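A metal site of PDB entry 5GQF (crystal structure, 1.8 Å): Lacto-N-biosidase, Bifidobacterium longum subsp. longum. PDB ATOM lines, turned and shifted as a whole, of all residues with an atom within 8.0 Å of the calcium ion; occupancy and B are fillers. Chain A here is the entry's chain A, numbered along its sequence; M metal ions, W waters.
The backbone carbonyl oxygen of Asp 209 sits at hydrogen-bond distance from the guanidinium group of Arg 179 (2.8 Å).
The backbone carbonyl oxygen of Asp 149 sits at hydrogen-bond distance from the guanidinium group of Arg 182, 3.1 Å away.
NH2 of Arg 182 is in salt-bridge range of OD2 of Asp 150 (3.6 Å).
N of Asp 149 is in hydrogen-bond range of O of Asp 207, 3.1 Å away.
The side-chain carboxylate of Asp 150 is in hydrogen-bond range of the backbone NH of Asp 152, at 2.9 Å.
NH2 of Arg 179 lies within salt-bridge range of OD2 of Asp 150 (2.8 Å).
N of Asp 209 lies within hydrogen-bond range of O of Asn 148 (2.9 Å).
The side-chain carboxylate (OD1) of Asp 149 binds the calcium ion, at 2.2 Å.
O of Val 153 binds the calcium ion.
OD2 of Asp 209 binds the calcium ion (2.3 Å).
The backbone carbonyl oxygen (O) of Asp 150 binds the calcium ion (2.5 Å).
Water W1 binds the calcium ion (2.5 Å).
The calcium ion is bound by water W2 (2.6 Å).
The calcium ion has six donor atoms within binding distance.
Water W1 lies within hydrogen-bond range of OD1 of Asp 207 and OD1 of Asp 209.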
ATOM      1  N   ASN A 103     -21.925 -21.441  23.514  1.00  0.00           N
ATOM      2  CA  ASN A 103     -22.474 -20.264  24.109  1.00  0.00           C
ATOM      3  C   ASN A 103     -21.523 -19.067  24.319  1.00  0.00           C
ATOM      4  O   ASN A 103     -21.638 -18.262  25.235  1.00  0.00           O
ATOM      5  CB  ASN A 103     -23.168 -20.598  25.450  1.00  0.00           C
ATOM      6  CG  ASN A 103     -24.185 -21.683  25.312  1.00  0.00           C
ATOM      7  OD1 ASN A 103     -24.976 -21.729  24.349  1.00  0.00           O
ATOM      8  ND2 ASN A 103     -24.175 -22.611  26.294  1.00  0.00           N
ATOM      9  N   ASN A 148     -23.670 -21.442  18.575  1.00  0.00           N
ATOM     10  CA  ASN A 148     -22.924 -20.460  19.327  1.00  0.00           C
ATOM     11  C   ASN A 148     -23.816 -19.315  19.735  1.00  0.00           C
ATOM     12  O   ASN A 148     -23.740 -18.147  19.275  1.00  0.00           O
ATOM     13  CB  ASN A 148     -21.739 -19.970  18.571  1.00  0.00           C
ATOM     14  CG  ASN A 148     -20.715 -19.278  19.494  1.00  0.00           C
ATOM     15  OD1 ASN A 148     -21.053 -18.797  20.549  1.00  0.00           O
ATOM     16  ND2 ASN A 148     -19.486 -19.149  19.032  1.00  0.00           N
ATOM     17  N   ASP A 149     -24.656 -19.655  20.702  1.00  0.00           N
ATOM     18  CA  ASP A 149     -25.836 -18.901  21.107  1.00  0.00           C
ATOM     19  C   ASP A 149     -25.623 -17.945  22.222  1.00  0.00           C
ATOM     20  O   ASP A 149     -24.817 -18.216  23.132  1.00  0.00           O
ATOM     21  CB  ASP A 149     -26.900 -19.983  21.400  1.00  0.00           C
ATOM     22  CG  ASP A 149     -28.193 -19.385  21.819  1.00  0.00           C
ATOM     23  OD1 ASP A 149     -28.739 -18.590  21.064  1.00  0.00           O
ATOM     24  OD2 ASP A 149     -28.624 -19.648  22.939  1.00  0.00           O
ATOM     25  N   ASP A 150     -26.297 -16.773  22.150  1.00  0.00           N
ATOM     26  CA  ASP A 150     -26.341 -15.795  23.170  1.00  0.00           C
ATOM     27  C   ASP A 150     -27.804 -15.854  23.567  1.00  0.00           C
ATOM     28  O   ASP A 150     -28.713 -15.706  22.737  1.00  0.00           O
ATOM     29  CB  ASP A 150     -25.949 -14.428  22.635  1.00  0.00           C
ATOM     30  CG  ASP A 150     -25.836 -13.397  23.679  1.00  0.00           C
ATOM     31  OD1 ASP A 150     -26.510 -13.549  24.728  1.00  0.00           O
ATOM     32  OD2 ASP A 150     -25.116 -12.392  23.438  1.00  0.00           O
ATOM     33  N   ALA A 151     -28.048 -16.031  24.884  1.00  0.00           N
ATOM     34  CA  ALA A 151     -29.410 -16.165  25.352  1.00  0.00           C
ATOM     35  C   ALA A 151     -30.112 -14.803  25.194  1.00  0.00           C
ATOM     36  O   ALA A 151     -31.318 -14.744  25.119  1.00  0.00           O
ATOM     37  CB  ALA A 151     -29.430 -16.680  26.803  1.00  0.00           C
ATOM     38  N   ASP A 152     -29.368 -13.704  25.213  1.00  0.00           N
ATOM     39  CA  ASP A 152     -29.966 -12.398  25.047  1.00  0.00           C
ATOM     40  C   ASP A 152     -30.165 -11.928  23.572  1.00  0.00           C
ATOM     41  O   ASP A 152     -30.480 -10.770  23.369  1.00  0.00           O
ATOM     42  CB  ASP A 152     -29.048 -11.369  25.682  1.00  0.00           C
ATOM     43  CG  ASP A 152     -28.916 -11.560  27.166  1.00  0.00           C
ATOM     44  OD1 ASP A 152     -29.788 -12.216  27.776  1.00  0.00           O
ATOM     45  OD2 ASP A 152     -27.926 -11.044  27.727  1.00  0.00           O
ATOM     46  N   VAL A 153     -29.940 -12.785  22.608  1.00  0.00           N
ATOM     47  CA  VAL A 153     -30.222 -12.467  21.214  1.00  0.00           C
ATOM     48  C   VAL A 153     -31.163 -13.521  20.705  1.00  0.00           C
ATOM     49  O   VAL A 153     -30.837 -14.741  20.740  1.00  0.00           O
ATOM     50  CB  VAL A 153     -28.900 -12.474  20.355  1.00  0.00           C
ATOM     51  CG1 VAL A 153     -29.169 -12.314  18.843  1.00  0.00           C
ATOM     52  CG2 VAL A 153     -27.934 -11.410  20.778  1.00  0.00           C
ATOM     53  N   TYR A 154     -32.316 -13.116  20.135  1.00  0.00           N
ATOM     54  CA  TYR A 154     -33.268 -14.055  19.678  1.00  0.00           C
ATOM     55  C   TYR A 154     -34.131 -13.412  18.554  1.00  0.00           C
ATOM     56  O   TYR A 154     -34.821 -12.405  18.808  1.00  0.00           O
ATOM     57  CB  TYR A 154     -34.176 -14.451  20.862  1.00  0.00           C
ATOM     58  CG  TYR A 154     -35.191 -15.481  20.486  1.00  0.00           C
ATOM     59  CD1 TYR A 154     -34.838 -16.793  20.260  1.00  0.00           C
ATOM     60  CD2 TYR A 154     -36.545 -15.134  20.304  1.00  0.00           C
ATOM     61  CE1 TYR A 154     -35.808 -17.744  19.910  1.00  0.00           C
ATOM     62  CE2 TYR A 154     -37.504 -16.083  19.946  1.00  0.00           C
ATOM     63  CZ  TYR A 154     -37.142 -17.382  19.784  1.00  0.00           C
ATOM     64  OH  TYR A 154     -38.112 -18.312  19.427  1.00  0.00           O
ATOM     65  N   ASP A 155     -34.035 -13.990  17.383  1.00  0.00           N
ATOM     66  CA  ASP A 155     -34.665 -13.425  16.209  1.00  0.00           C
ATOM     67  C   ASP A 155     -34.787 -14.495  15.159  1.00  0.00           C
ATOM     68  O   ASP A 155     -34.203 -14.390  14.049  1.00  0.00           O
ATOM     69  CB  ASP A 155     -33.850 -12.259  15.707  1.00  0.00           C
ATOM     70  CG  ASP A 155     -34.667 -11.340  14.754  1.00  0.00           C
ATOM     71  OD1 ASP A 155     -35.933 -11.441  14.742  1.00  0.00           O
ATOM     72  OD2 ASP A 155     -33.986 -10.497  14.121  1.00  0.00           O
ATOM     73  N   PRO A 156     -35.539 -15.569  15.469  1.00  0.00           N
ATOM     74  CA  PRO A 156     -35.637 -16.685  14.571  1.00  0.00           C
ATOM     75  C   PRO A 156     -36.252 -16.406  13.165  1.00  0.00           C
ATOM     76  O   PRO A 156     -37.283 -15.757  13.084  1.00  0.00           O
ATOM     77  CB  PRO A 156     -36.558 -17.668  15.310  1.00  0.00           C
ATOM     78  CG  PRO A 156     -37.363 -16.803  16.213  1.00  0.00           C
ATOM     79  CD  PRO A 156     -36.437 -15.700  16.633  1.00  0.00           C
ATOM     80  N   LYS A 172     -35.090  -9.973  20.287  1.00  0.00           N
ATOM     81  CA  LYS A 172     -34.096  -9.105  20.856  1.00  0.00           C
ATOM     82  C   LYS A 172     -32.733  -9.265  20.121  1.00  0.00           C
ATOM     83  O   LYS A 172     -32.342 -10.327  19.725  1.00  0.00           O
ATOM     84  CB  LYS A 172     -33.888  -9.359  22.377  1.00  0.00           C
ATOM     85  CG  LYS A 172     -33.961 -10.816  22.724  1.00  0.00           C
ATOM     86  CD  LYS A 172     -34.216 -11.143  24.226  1.00  0.00           C
ATOM     87  CE  LYS A 172     -34.419 -12.643  24.453  1.00  0.00           C
ATOM     88  NZ  LYS A 172     -35.760 -13.083  23.920  1.00  0.00           N
ATOM     89  N   ARG A 179     -19.829  -5.795  19.174  1.00  0.00           N
ATOM     90  CA  ARG A 179     -20.255  -7.117  19.555  1.00  0.00           C
ATOM     91  C   ARG A 179     -19.175  -8.137  19.164  1.00  0.00           C
ATOM     92  O   ARG A 179     -18.659  -8.103  18.044  1.00  0.00           O
ATOM     93  CB  ARG A 179     -21.641  -7.455  18.985  1.00  0.00           C
ATOM     94  CG  ARG A 179     -22.067  -8.879  19.201  1.00  0.00           C
ATOM     95  CD  ARG A 179     -23.487  -9.254  18.876  1.00  0.00           C
ATOM     96  NE  ARG A 179     -23.786 -10.636  19.292  1.00  0.00           N
ATOM     97  CZ  ARG A 179     -24.059 -11.019  20.560  1.00  0.00           C
ATOM     98  NH1 ARG A 179     -24.236 -10.141  21.535  1.00  0.00           N
ATOM     99  NH2 ARG A 179     -24.266 -12.288  20.791  1.00  0.00           N
ATOM    100  N   ARG A 182     -18.470 -14.158  16.272  1.00  0.00           N
ATOM    101  CA  ARG A 182     -18.687 -15.565  16.568  1.00  0.00           C
ATOM    102  C   ARG A 182     -18.816 -16.423  15.315  1.00  0.00           C
ATOM    103  O   ARG A 182     -19.445 -16.027  14.318  1.00  0.00           O
ATOM    104  CB  ARG A 182     -19.925 -15.796  17.425  1.00  0.00           C
ATOM    105  CG  ARG A 182     -20.059 -14.976  18.677  1.00  0.00           C
ATOM    106  CD  ARG A 182     -21.155 -15.548  19.563  1.00  0.00           C
ATOM    107  NE  ARG A 182     -21.406 -14.799  20.787  1.00  0.00           N
ATOM    108  CZ  ARG A 182     -22.088 -15.265  21.850  1.00  0.00           C
ATOM    109  NH1 ARG A 182     -22.594 -16.512  21.877  1.00  0.00           N
ATOM    110  NH2 ARG A 182     -22.279 -14.471  22.854  1.00  0.00           N
ATOM    111  N   HIS A 206     -26.418 -23.639  13.735  1.00  0.00           N
ATOM    112  CA  HIS A 206     -27.492 -22.654  13.980  1.00  0.00           C
ATOM    113  C   HIS A 206     -27.317 -21.882  15.210  1.00  0.00           C
ATOM    114  O   HIS A 206     -26.591 -22.296  16.121  1.00  0.00           O
ATOM    115  CB  HIS A 206     -28.856 -23.338  13.937  1.00  0.00           C
ATOM    116  CG  HIS A 206     -29.125 -24.319  15.057  1.00  0.00           C
ATOM    117  ND1 HIS A 206     -29.758 -23.950  16.232  1.00  0.00           N
ATOM    118  CD2 HIS A 206     -28.834 -25.640  15.177  1.00  0.00           C
ATOM    119  CE1 HIS A 206     -29.857 -25.004  17.038  1.00  0.00           C
ATOM    120  NE2 HIS A 206     -29.305 -26.048  16.417  1.00  0.00           N
ATOM    121  N   ASP A 207     -27.974 -20.733  15.272  1.00  0.00           N
ATOM    122  CA  ASP A 207     -27.932 -19.848  16.440  1.00  0.00           C
ATOM    123  C   ASP A 207     -26.513 -19.504  16.771  1.00  0.00           C
ATOM    124  O   ASP A 207     -26.014 -19.739  17.917  1.00  0.00           O
ATOM    125  CB  ASP A 207     -28.759 -20.499  17.590  1.00  0.00           C
ATOM    126  CG  ASP A 207     -30.196 -20.493  17.273  1.00  0.00           C
ATOM    127  OD1 ASP A 207     -30.827 -19.408  17.475  1.00  0.00           O
ATOM    128  OD2 ASP A 207     -30.713 -21.508  16.721  1.00  0.00           O
ATOM    129  N   VAL A 208     -25.828 -18.982  15.746  1.00  0.00           N
ATOM    130  CA  VAL A 208     -24.500 -18.410  15.892  1.00  0.00           C
ATOM    131  C   VAL A 208     -24.695 -16.945  15.958  1.00  0.00           C
ATOM    132  O   VAL A 208     -24.850 -16.276  14.902  1.00  0.00           O
ATOM    133  CB  VAL A 208     -23.528 -18.822  14.752  1.00  0.00           C
ATOM    134  CG1 VAL A 208     -22.156 -18.172  14.926  1.00  0.00           C
ATOM    135  CG2 VAL A 208     -23.383 -20.344  14.630  1.00  0.00           C
ATOM    136  N   ASP A 209     -24.677 -16.367  17.170  1.00  0.00           N
ATOM    137  CA  ASP A 209     -25.140 -15.006  17.382  1.00  0.00           C
ATOM    138  C   ASP A 209     -23.947 -14.058  17.341  1.00  0.00           C
ATOM    139  O   ASP A 209     -23.581 -13.413  18.306  1.00  0.00           O
ATOM    140  CB  ASP A 209     -25.934 -14.907  18.682  1.00  0.00           C
ATOM    141  CG  ASP A 209     -27.227 -15.670  18.643  1.00  0.00           C
ATOM    142  OD1 ASP A 209     -27.825 -15.833  17.517  1.00  0.00           O
ATOM    143  OD2 ASP A 209     -27.682 -16.027  19.789  1.00  0.00           O
ATOM    144  N   ASP A 260     -30.029 -19.092  11.083  1.00  0.00           N
ATOM    145  CA  ASP A 260     -30.045 -18.212  12.179  1.00  0.00           C
ATOM    146  C   ASP A 260     -28.634 -17.902  12.730  1.00  0.00           C
ATOM    147  O   ASP A 260     -28.297 -18.223  13.878  1.00  0.00           O
ATOM    148  CB  ASP A 260     -31.000 -18.688  13.346  1.00  0.00           C
ATOM    149  CG  ASP A 260     -32.480 -18.512  13.030  1.00  0.00           C
ATOM    150  OD1 ASP A 260     -32.873 -17.589  12.265  1.00  0.00           O
ATOM    151  OD2 ASP A 260     -33.275 -19.312  13.505  1.00  0.00           O
HETATM  152 CA    CA M   1     -29.738 -16.674  20.711  1.00  0.00          CA
HETATM  153  O   HOH W   1     -30.195 -17.003  18.243  1.00  0.00           O
HETATM  154  O   HOH W   2     -31.574 -17.070  22.475  1.00  0.00           O
